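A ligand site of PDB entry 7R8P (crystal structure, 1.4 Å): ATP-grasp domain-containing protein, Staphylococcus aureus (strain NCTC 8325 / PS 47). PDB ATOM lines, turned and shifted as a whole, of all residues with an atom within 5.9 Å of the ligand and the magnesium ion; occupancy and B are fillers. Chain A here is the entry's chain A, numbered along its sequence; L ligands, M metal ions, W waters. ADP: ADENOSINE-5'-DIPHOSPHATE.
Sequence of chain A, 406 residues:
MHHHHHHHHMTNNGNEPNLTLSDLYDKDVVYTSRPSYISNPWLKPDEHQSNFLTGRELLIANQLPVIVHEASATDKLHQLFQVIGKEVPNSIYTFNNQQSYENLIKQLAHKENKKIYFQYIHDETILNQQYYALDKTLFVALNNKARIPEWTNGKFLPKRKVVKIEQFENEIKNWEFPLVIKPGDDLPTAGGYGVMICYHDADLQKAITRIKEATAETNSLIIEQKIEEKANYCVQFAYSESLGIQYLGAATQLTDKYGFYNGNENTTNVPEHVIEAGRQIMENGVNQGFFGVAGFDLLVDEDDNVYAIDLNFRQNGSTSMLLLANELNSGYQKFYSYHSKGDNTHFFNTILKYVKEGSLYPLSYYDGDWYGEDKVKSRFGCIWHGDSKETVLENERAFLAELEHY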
ATOM      1  N   LYS A 145       7.575  31.919 -16.047  1.00  0.00           N
ATOM      2  CA  LYS A 145       7.330  31.053 -17.192  1.00  0.00           C
ATOM      3  C   LYS A 145       5.888  30.586 -17.268  1.00  0.00           C
ATOM      4  O   LYS A 145       5.369  30.310 -18.360  1.00  0.00           O
ATOM      5  CB  LYS A 145       8.305  29.870 -17.181  1.00  0.00           C
ATOM      6  CG  LYS A 145       8.605  29.296 -18.553  1.00  0.00           C
ATOM      7  CD  LYS A 145       9.750  28.266 -18.516  1.00  0.00           C
ATOM      8  CE  LYS A 145      11.115  28.926 -18.473  1.00  0.00           C
ATOM      9  NZ  LYS A 145      12.226  27.942 -18.593  1.00  0.00           N
ATOM     10  N   PRO A 158       3.009  26.134 -27.716  1.00  0.00           N
ATOM     11  CA  PRO A 158       2.769  24.691 -27.871  1.00  0.00           C
ATOM     12  C   PRO A 158       1.612  24.269 -26.993  1.00  0.00           C
ATOM     13  O   PRO A 158       1.144  25.030 -26.136  1.00  0.00           O
ATOM     14  CB  PRO A 158       4.083  24.072 -27.385  1.00  0.00           C
ATOM     15  CG  PRO A 158       4.640  25.066 -26.442  1.00  0.00           C
ATOM     16  CD  PRO A 158       4.164  26.423 -26.859  1.00  0.00           C
ATOM     17  N   VAL A 180       7.938  18.072 -22.200  1.00  0.00           N
ATOM     18  CA  VAL A 180       8.842  18.824 -21.327  1.00  0.00           C
ATOM     19  C   VAL A 180       8.110  19.184 -20.047  1.00  0.00           C
ATOM     20  O   VAL A 180       6.967  19.640 -20.081  1.00  0.00           O
ATOM     21  CB  VAL A 180       9.339  20.116 -22.017  1.00  0.00           C
ATOM     22  CG1 VAL A 180      10.476  20.722 -21.226  1.00  0.00           C
ATOM     23  CG2 VAL A 180       9.759  19.839 -23.461  1.00  0.00           C
ATOM     24  N   LYS A 182       8.543  21.607 -16.627  1.00  0.00           N
ATOM     25  CA  LYS A 182       9.288  22.744 -16.110  1.00  0.00           C
ATOM     26  C   LYS A 182       8.702  23.201 -14.779  1.00  0.00           C
ATOM     27  O   LYS A 182       7.505  23.054 -14.545  1.00  0.00           O
ATOM     28  CB  LYS A 182       9.222  23.920 -17.096  1.00  0.00           C
ATOM     29  CG  LYS A 182       9.567  23.558 -18.531  1.00  0.00           C
ATOM     30  CD  LYS A 182       9.632  24.776 -19.430  1.00  0.00           C
ATOM     31  CE  LYS A 182       9.861  24.331 -20.867  1.00  0.00           C
ATOM     32  NZ  LYS A 182      10.003  25.491 -21.789  1.00  0.00           N
ATOM     33  N   VAL A 195      14.438  22.235 -16.146  1.00  0.00           N
ATOM     34  CA  VAL A 195      13.664  21.719 -17.275  1.00  0.00           C
ATOM     35  C   VAL A 195      14.004  20.253 -17.481  1.00  0.00           C
ATOM     36  O   VAL A 195      15.173  19.865 -17.545  1.00  0.00           O
ATOM     37  CB  VAL A 195      14.001  22.547 -18.529  1.00  0.00           C
ATOM     38  CG1 VAL A 195      13.559  21.843 -19.795  1.00  0.00           C
ATOM     39  CG2 VAL A 195      13.388  23.941 -18.419  1.00  0.00           C
ATOM     40  N   ILE A 197      13.205  17.363 -20.139  1.00  0.00           N
ATOM     41  CA  ILE A 197      12.674  16.837 -21.395  1.00  0.00           C
ATOM     42  C   ILE A 197      12.594  15.320 -21.299  1.00  0.00           C
ATOM     43  O   ILE A 197      13.545  14.659 -20.863  1.00  0.00           O
ATOM     44  CB  ILE A 197      13.557  17.284 -22.571  1.00  0.00           C
ATOM     45  CG1 ILE A 197      13.626  18.817 -22.619  1.00  0.00           C
ATOM     46  CG2 ILE A 197      13.024  16.731 -23.895  1.00  0.00           C
ATOM     47  CD1 ILE A 197      14.346  19.372 -23.829  1.00  0.00           C
ATOM     48  N   GLU A 224       4.645  20.745 -21.256  1.00  0.00           N
ATOM     49  CA  GLU A 224       4.628  21.335 -22.589  1.00  0.00           C
ATOM     50  C   GLU A 224       4.948  20.254 -23.613  1.00  0.00           C
ATOM     51  O   GLU A 224       5.821  19.416 -23.369  1.00  0.00           O
ATOM     52  CB  GLU A 224       5.710  22.409 -22.625  1.00  0.00           C
ATOM     53  CG  GLU A 224       5.481  23.566 -23.520  1.00  0.00           C
ATOM     54  CD  GLU A 224       6.450  24.691 -23.240  1.00  0.00           C
ATOM     55  OE1 GLU A 224       7.671  24.477 -23.354  1.00  0.00           O
ATOM     56  OE2 GLU A 224       5.993  25.790 -22.874  1.00  0.00           O
ATOM     57  N   GLN A 225       4.279  20.274 -24.760  1.00  0.00           N
ATOM     58  CA  GLN A 225       4.723  19.390 -25.834  1.00  0.00           C
ATOM     59  C   GLN A 225       6.130  19.781 -26.284  1.00  0.00           C
ATOM     60  O   GLN A 225       6.439  20.969 -26.391  1.00  0.00           O
ATOM     61  CB  GLN A 225       3.744  19.407 -27.014  1.00  0.00           C
ATOM     62  CG  GLN A 225       3.838  20.602 -27.920  1.00  0.00           C
ATOM     63  CD  GLN A 225       2.941  20.479 -29.124  1.00  0.00           C
ATOM     64  OE1 GLN A 225       2.195  21.401 -29.446  1.00  0.00           O
ATOM     65  NE2 GLN A 225       3.010  19.340 -29.813  1.00  0.00           N
ATOM     66  N   LYS A 226       6.982  18.784 -26.496  1.00  0.00           N
ATOM     67  CA  LYS A 226       8.331  19.040 -27.021  1.00  0.00           C
ATOM     68  C   LYS A 226       8.200  19.216 -28.522  1.00  0.00           C
ATOM     69  O   LYS A 226       7.863  18.281 -29.257  1.00  0.00           O
ATOM     70  CB  LYS A 226       9.283  17.907 -26.654  1.00  0.00           C
ATOM     71  CG  LYS A 226      10.773  18.282 -26.748  1.00  0.00           C
ATOM     72  CD  LYS A 226      11.284  18.182 -28.170  1.00  0.00           C
ATOM     73  CE  LYS A 226      12.761  18.529 -28.252  1.00  0.00           C
ATOM     74  NZ  LYS A 226      13.133  18.752 -29.671  1.00  0.00           N
ATOM     75  N   ILE A 227       8.449  20.449 -28.987  1.00  0.00           N
ATOM     76  CA  ILE A 227       8.426  20.770 -30.401  1.00  0.00           C
ATOM     77  C   ILE A 227       9.663  20.180 -31.076  1.00  0.00           C
ATOM     78  O   ILE A 227      10.782  20.273 -30.560  1.00  0.00           O
ATOM     79  CB  ILE A 227       8.417  22.297 -30.550  1.00  0.00           C
ATOM     80  CG1 ILE A 227       7.189  22.889 -29.844  1.00  0.00           C
ATOM     81  CG2 ILE A 227       8.480  22.695 -32.022  1.00  0.00           C
ATOM     82  CD1 ILE A 227       5.864  22.394 -30.389  1.00  0.00           C
ATOM     83  N   GLU A 228       9.455  19.571 -32.249  1.00  0.00           N
ATOM     84  CA  GLU A 228      10.559  19.045 -33.063  1.00  0.00           C
ATOM     85  C   GLU A 228      11.061  20.198 -33.919  1.00  0.00           C
ATOM     86  O   GLU A 228      10.673  20.379 -35.081  1.00  0.00           O
ATOM     87  CB  GLU A 228      10.069  17.885 -33.917  1.00  0.00           C
ATOM     88  CG  GLU A 228      11.088  16.816 -34.220  1.00  0.00           C
ATOM     89  CD  GLU A 228      10.499  15.677 -35.036  1.00  0.00           C
ATOM     90  OE1 GLU A 228      10.401  15.820 -36.271  1.00  0.00           O
ATOM     91  OE2 GLU A 228      10.100  14.650 -34.434  1.00  0.00           O
ATOM     92  N   GLU A 229      11.915  21.023 -33.326  1.00  0.00           N
ATOM     93  CA  GLU A 229      12.239  22.281 -33.975  1.00  0.00           C
ATOM     94  C   GLU A 229      13.247  22.051 -35.095  1.00  0.00           C
ATOM     95  O   GLU A 229      14.079  21.145 -35.035  1.00  0.00           O
ATOM     96  CB  GLU A 229      12.767  23.304 -32.965  1.00  0.00           C
ATOM     97  CG  GLU A 229      14.195  23.062 -32.469  1.00  0.00           C
ATOM     98  CD  GLU A 229      14.262  22.118 -31.287  1.00  0.00           C
ATOM     99  OE1 GLU A 229      15.338  22.036 -30.652  1.00  0.00           O
ATOM    100  OE2 GLU A 229      13.252  21.464 -30.975  1.00  0.00           O
ATOM    101  N   GLN A 253      20.654  29.097 -30.053  1.00  0.00           N
ATOM    102  CA  GLN A 253      21.017  28.411 -28.826  1.00  0.00           C
ATOM    103  C   GLN A 253      21.515  27.019 -29.169  1.00  0.00           C
ATOM    104  O   GLN A 253      20.850  26.286 -29.911  1.00  0.00           O
ATOM    105  CB  GLN A 253      19.830  28.302 -27.871  1.00  0.00           C
ATOM    106  CG  GLN A 253      19.147  29.614 -27.541  1.00  0.00           C
ATOM    107  CD  GLN A 253      18.193  29.463 -26.369  1.00  0.00           C
ATOM    108  OE1 GLN A 253      18.589  29.563 -25.218  1.00  0.00           O
ATOM    109  NE2 GLN A 253      16.919  29.213 -26.668  1.00  0.00           N
ATOM    110  N   THR A 255      21.927  23.590 -27.648  1.00  0.00           N
ATOM    111  CA  THR A 255      21.482  22.774 -26.527  1.00  0.00           C
ATOM    112  C   THR A 255      21.546  21.315 -26.929  1.00  0.00           C
ATOM    113  O   THR A 255      21.325  20.979 -28.101  1.00  0.00           O
ATOM    114  CB  THR A 255      20.041  23.077 -26.115  1.00  0.00           C
ATOM    115  OG1 THR A 255      19.174  22.832 -27.224  1.00  0.00           O
ATOM    116  CG2 THR A 255      19.885  24.518 -25.662  1.00  0.00           C
ATOM    117  N   ASP A 256      21.833  20.453 -25.965  1.00  0.00           N
ATOM    118  CA  ASP A 256      21.725  19.020 -26.230  1.00  0.00           C
ATOM    119  C   ASP A 256      20.257  18.629 -26.275  1.00  0.00           C
ATOM    120  O   ASP A 256      19.346  19.451 -26.135  1.00  0.00           O
ATOM    121  CB  ASP A 256      22.596  18.201 -25.265  1.00  0.00           C
ATOM    122  CG  ASP A 256      22.090  18.221 -23.824  1.00  0.00           C
ATOM    123  OD1 ASP A 256      20.926  18.599 -23.567  1.00  0.00           O
ATOM    124  OD2 ASP A 256      22.849  17.825 -22.926  1.00  0.00           O
ATOM    125  N   TYR A 258      18.434  17.208 -24.257  1.00  0.00           N
ATOM    126  CA  TYR A 258      17.733  17.422 -23.001  1.00  0.00           C
ATOM    127  C   TYR A 258      17.651  18.900 -22.632  1.00  0.00           C
ATOM    128  O   TYR A 258      17.221  19.232 -21.517  1.00  0.00           O
ATOM    129  CB  TYR A 258      18.360  16.585 -21.885  1.00  0.00           C
ATOM    130  CG  TYR A 258      17.997  15.121 -22.040  1.00  0.00           C
ATOM    131  CD1 TYR A 258      16.711  14.693 -21.756  1.00  0.00           C
ATOM    132  CD2 TYR A 258      18.926  14.174 -22.478  1.00  0.00           C
ATOM    133  CE1 TYR A 258      16.348  13.371 -21.895  1.00  0.00           C
ATOM    134  CE2 TYR A 258      18.562  12.842 -22.616  1.00  0.00           C
ATOM    135  CZ  TYR A 258      17.268  12.446 -22.326  1.00  0.00           C
ATOM    136  OH  TYR A 258      16.885  11.126 -22.456  1.00  0.00           O
ATOM    137  N   GLY A 259      18.027  19.803 -23.542  1.00  0.00           N
ATOM    138  CA  GLY A 259      17.885  21.228 -23.329  1.00  0.00           C
ATOM    139  C   GLY A 259      19.015  21.880 -22.573  1.00  0.00           C
ATOM    140  O   GLY A 259      18.896  23.072 -22.264  1.00  0.00           O
ATOM    141  N   PHE A 260      20.085  21.157 -22.270  1.00  0.00           N
ATOM    142  CA  PHE A 260      21.193  21.759 -21.529  1.00  0.00           C
ATOM    143  C   PHE A 260      22.001  22.688 -22.407  1.00  0.00           C
ATOM    144  O   PHE A 260      22.274  22.390 -23.578  1.00  0.00           O
ATOM    145  CB  PHE A 260      22.063  20.672 -20.895  1.00  0.00           C
ATOM    146  CG  PHE A 260      21.351  19.887 -19.841  1.00  0.00           C
ATOM    147  CD1 PHE A 260      20.931  18.589 -20.075  1.00  0.00           C
ATOM    148  CD2 PHE A 260      21.074  20.455 -18.599  1.00  0.00           C
ATOM    149  CE1 PHE A 260      20.264  17.863 -19.097  1.00  0.00           C
ATOM    150  CE2 PHE A 260      20.408  19.740 -17.622  1.00  0.00           C
ATOM    151  CZ  PHE A 260      19.998  18.448 -17.876  1.00  0.00           C
ATOM    152  N   ASP A 297      13.306  33.100 -26.334  1.00  0.00           N
ATOM    153  CA  ASP A 297      13.665  31.811 -26.932  1.00  0.00           C
ATOM    154  C   ASP A 297      12.510  31.368 -27.812  1.00  0.00           C
ATOM    155  O   ASP A 297      11.442  30.960 -27.306  1.00  0.00           O
ATOM    156  CB  ASP A 297      13.896  30.732 -25.874  1.00  0.00           C
ATOM    157  CG  ASP A 297      15.059  31.007 -24.955  1.00  0.00           C
ATOM    158  OD1 ASP A 297      15.662  32.102 -24.989  1.00  0.00           O
ATOM    159  OD2 ASP A 297      15.366  30.084 -24.176  1.00  0.00           O
ATOM    160  N   LEU A 299      11.298  28.917 -30.946  1.00  0.00           N
ATOM    161  CA  LEU A 299      11.539  27.751 -31.780  1.00  0.00           C
ATOM    162  C   LEU A 299      10.707  27.848 -33.048  1.00  0.00           C
ATOM    163  O   LEU A 299       9.623  28.445 -33.046  1.00  0.00           O
ATOM    164  CB  LEU A 299      11.112  26.478 -31.051  1.00  0.00           C
ATOM    165  CG  LEU A 299      11.631  26.234 -29.649  1.00  0.00           C
ATOM    166  CD1 LEU A 299      11.125  24.901 -29.146  1.00  0.00           C
ATOM    167  CD2 LEU A 299      13.147  26.277 -29.627  1.00  0.00           C
ATOM    168  N   ILE A 309       8.996  29.622 -26.010  1.00  0.00           N
ATOM    169  CA  ILE A 309       9.103  28.644 -24.934  1.00  0.00           C
ATOM    170  C   ILE A 309       9.709  29.237 -23.665  1.00  0.00           C
ATOM    171  O   ILE A 309       9.589  28.626 -22.593  1.00  0.00           O
ATOM    172  CB  ILE A 309       9.893  27.403 -25.382  1.00  0.00           C
ATOM    173  CG1 ILE A 309      11.263  27.832 -25.876  1.00  0.00           C
ATOM    174  CG2 ILE A 309       9.110  26.611 -26.460  1.00  0.00           C
ATOM    175  CD1 ILE A 309      12.284  26.713 -25.902  1.00  0.00           C
ATOM    176  N   ASP A 310      10.367  30.392 -23.765  1.00  0.00           N
ATOM    177  CA  ASP A 310      11.044  30.967 -22.613  1.00  0.00           C
ATOM    178  C   ASP A 310      11.215  32.446 -22.905  1.00  0.00           C
ATOM    179  O   ASP A 310      11.809  32.809 -23.924  1.00  0.00           O
ATOM    180  CB  ASP A 310      12.409  30.281 -22.431  1.00  0.00           C
ATOM    181  CG  ASP A 310      13.215  30.828 -21.274  1.00  0.00           C
ATOM    182  OD1 ASP A 310      12.612  31.383 -20.347  1.00  0.00           O
ATOM    183  OD2 ASP A 310      14.461  30.709 -21.327  1.00  0.00           O
ATOM    184  N   ASN A 312      12.907  35.923 -21.519  1.00  0.00           N
ATOM    185  CA  ASN A 312      13.932  36.390 -20.593  1.00  0.00           C
ATOM    186  C   ASN A 312      13.932  37.915 -20.661  1.00  0.00           C
ATOM    187  O   ASN A 312      14.616  38.493 -21.501  1.00  0.00           O
ATOM    188  CB  ASN A 312      15.274  35.795 -20.974  1.00  0.00           C
ATOM    189  CG  ASN A 312      15.227  34.283 -20.999  1.00  0.00           C
ATOM    190  OD1 ASN A 312      15.156  33.646 -19.954  1.00  0.00           O
ATOM    191  ND2 ASN A 312      15.222  33.709 -22.193  1.00  0.00           N
ATOM    192  N   ARG A 314      15.457  40.332 -19.391  1.00  0.00           N
ATOM    193  CA  ARG A 314      16.770  40.513 -18.782  1.00  0.00           C
ATOM    194  C   ARG A 314      17.740  40.154 -19.898  1.00  0.00           C
ATOM    195  O   ARG A 314      17.326  39.644 -20.943  1.00  0.00           O
ATOM    196  CB  ARG A 314      16.949  39.595 -17.572  1.00  0.00           C
ATOM    197  CG  ARG A 314      16.659  38.120 -17.875  1.00  0.00           C
ATOM    198  CD  ARG A 314      16.679  37.249 -16.611  1.00  0.00           C
ATOM    199  NE  ARG A 314      16.305  35.870 -16.906  1.00  0.00           N
ATOM    200  CZ  ARG A 314      17.190  34.906 -17.161  1.00  0.00           C
ATOM    201  NH1 ARG A 314      18.489  35.164 -17.145  1.00  0.00           N
ATOM    202  NH2 ARG A 314      16.764  33.676 -17.423  1.00  0.00           N
HETATM  203  PB  ADP L   1      15.696  27.910 -19.344  1.00  0.00           P
HETATM  204  O1B ADP L   1      16.657  27.035 -18.562  1.00  0.00           O
HETATM  205  O2B ADP L   1      14.856  28.807 -18.477  1.00  0.00           O
HETATM  206  O3B ADP L   1      16.297  28.649 -20.515  1.00  0.00           O
HETATM  207  PA  ADP L   1      13.945  26.747 -21.359  1.00  0.00           P
HETATM  208  O1A ADP L   1      14.499  27.754 -22.319  1.00  0.00           O
HETATM  209  O2A ADP L   1      12.455  26.709 -21.140  1.00  0.00           O
HETATM  210  O3A ADP L   1      14.644  26.818 -19.920  1.00  0.00           O
HETATM  211  O5' ADP L   1      14.341  25.283 -21.876  1.00  0.00           O
HETATM  212  C5' ADP L   1      15.730  25.003 -22.111  1.00  0.00           C
HETATM  213  C4' ADP L   1      15.858  24.408 -23.503  1.00  0.00           C
HETATM  214  O4' ADP L   1      15.062  23.223 -23.582  1.00  0.00           O
HETATM  215  C3' ADP L   1      15.384  25.271 -24.660  1.00  0.00           C
HETATM  216  O3' ADP L   1      16.386  26.216 -25.085  1.00  0.00           O
HETATM  217  C2' ADP L   1      15.078  24.247 -25.728  1.00  0.00           C
HETATM  218  O2' ADP L   1      16.290  23.756 -26.344  1.00  0.00           O
HETATM  219  C1' ADP L   1      14.537  23.103 -24.903  1.00  0.00           C
HETATM  220  N9  ADP L   1      13.069  23.215 -24.772  1.00  0.00           N
HETATM  221  C8  ADP L   1      12.391  23.729 -23.719  1.00  0.00           C
HETATM  222  N7  ADP L   1      11.047  23.655 -23.918  1.00  0.00           N
HETATM  223  C5  ADP L   1      10.882  23.080 -25.124  1.00  0.00           C
HETATM  224  C6  ADP L   1       9.740  22.692 -25.960  1.00  0.00           C
HETATM  225  N6  ADP L   1       8.472  22.906 -25.515  1.00  0.00           N
HETATM  226  N1  ADP L   1       9.976  22.123 -27.142  1.00  0.00           N
HETATM  227  C2  ADP L   1      11.232  21.890 -27.584  1.00  0.00           C
HETATM  228  N3  ADP L   1      12.322  22.217 -26.884  1.00  0.00           N
HETATM  229  C4  ADP L   1      12.207  22.801 -25.672  1.00  0.00           C
HETATM  230 MG    MG M   1      15.784  29.327 -22.367  1.00  0.00          MG
HETATM  231  O   HOH W   1      14.636  31.565 -17.556  1.00  0.00           O
HETATM  232  O   HOH W   2      17.346  30.787 -22.077  1.00  0.00           O
HETATM  233  O   HOH W   3      17.282  28.050 -23.265  1.00  0.00           O
HETATM  234  O   HOH W   4      14.840  21.730 -28.139  1.00  0.00           O
HETATM  235  O   HOH W   5      14.599  28.671 -15.929  1.00  0.00           O
HETATM  236  O   HOH W   6      16.115  25.588 -16.547  1.00  0.00           O
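The magnesium ion is bound by OD2 of Asp 297 (2.0 Å). O1A of the ligand is bound to the magnesium ion. The magnesium ion is bound by O3B of the ligand (2.0 Å). Water W2 binds the magnesium ion (2.2 Å). Water W3 binds the magnesium ion, 2.2 Å away. OD2 of Asp 310 binds the magnesium ion (2.2 Å).
Water W3 bridges O3' of the ligand (2.7 Å) and OE1 of Gln 253 (2.8 Å). Water W4 bridges the side-chain carboxylate of Glu 229 and a nitrogen (N3) of the ligand. Water W1 lies within hydrogen-bond range of an oxygen (O2B) of the ligand, the guanidinium group of Arg 314, the side-chain amide oxygen of Asn 312 and the side-chain carboxylate of Asp 310.
CG2 of Val 180 touches C6 of the ligand, at 3.8 Å. Val 195 touches the ligand (CG2 to O3A, 3.5 Å). Ile 197 touches the ligand (CD1 to C1', 3.9 Å). Lys 226 touches the ligand (CA to N1, 3.5 Å). OE2 of Glu 229 touches C2 of the ligand, at 3.97 Å. CA of Gly 259 touches O4' of the ligand, 3.5 Å away. Leu 299 touches the ligand. Ile 309 touches the ligand. Hydrophobic or aromatic side chains that line the ligand: Val 180, Val 195, Ile 197, Ile 227, Leu 299 and Ile 309. Of the 24 residues printed, 17 come within 4 Å of the ligand. Along chain A the residues within 4 Å of the ligand span positions 145 to 310. The nearest printed residue that does not touch the ligand is Pro 158 (4.5 Å).
ND2 of Asn 312 lies within hydrogen-bond range of OD1 of Asp 297 (3.3 Å). O of Asp 297 is in hydrogen-bond range of N of Ile 309. NZ of Lys 182 is in salt-bridge range of OE1 of Glu 224 (3.0 Å). The side-chain carboxylate of Asp 310 sits close to the side-chain amide oxygen of Asn 312, at 3.4 Å. OD1 of Asp 310 lies within salt-bridge range of NZ of Lys 145 (3.9 Å). N of Val 180 is in hydrogen-bond range of O of Glu 224 (2.8 Å). NZ of Lys 182 is in hydrogen-bond range of O of Ile 309 (3.3 Å). The side-chain amino group (NZ) of Lys 226 is in salt-bridge range of the side-chain carboxylate (OE2) of Glu 229 (3.0 Å).
NE2 of Gln 253 lies within hydrogen-bond range of O3' of the ligand. The side-chain amino group (NZ) of Lys 182 is in salt-bridge range of an oxygen (O2A) of the ligand. The backbone NH (N) of Ile 227 sits at hydrogen-bond distance from a nitrogen (N1) of the ligand, at 2.9 Å. A nitrogen (N6) of the ligand sits at hydrogen-bond distance from the side-chain carboxylate of Glu 224 (2.8 Å). O of Gln 225 is in hydrogen-bond range of N6 of the ligand, 2.9 Å away. The side-chain hydroxyl (OG1) of Thr 255 sits at hydrogen-bond distance from an oxygen (O2') of the ligand, 3.2 Å away. The side-chain amino group of Lys 145 lies within salt-bridge range of an oxygen (O2B) of the ligand (2.8 Å).
Within 4 Å of the magnesium ion: Asp 297 and Asp 310. The nearest printed residue that does not touch the magnesium ion is Gln 253 (4.01 Å).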
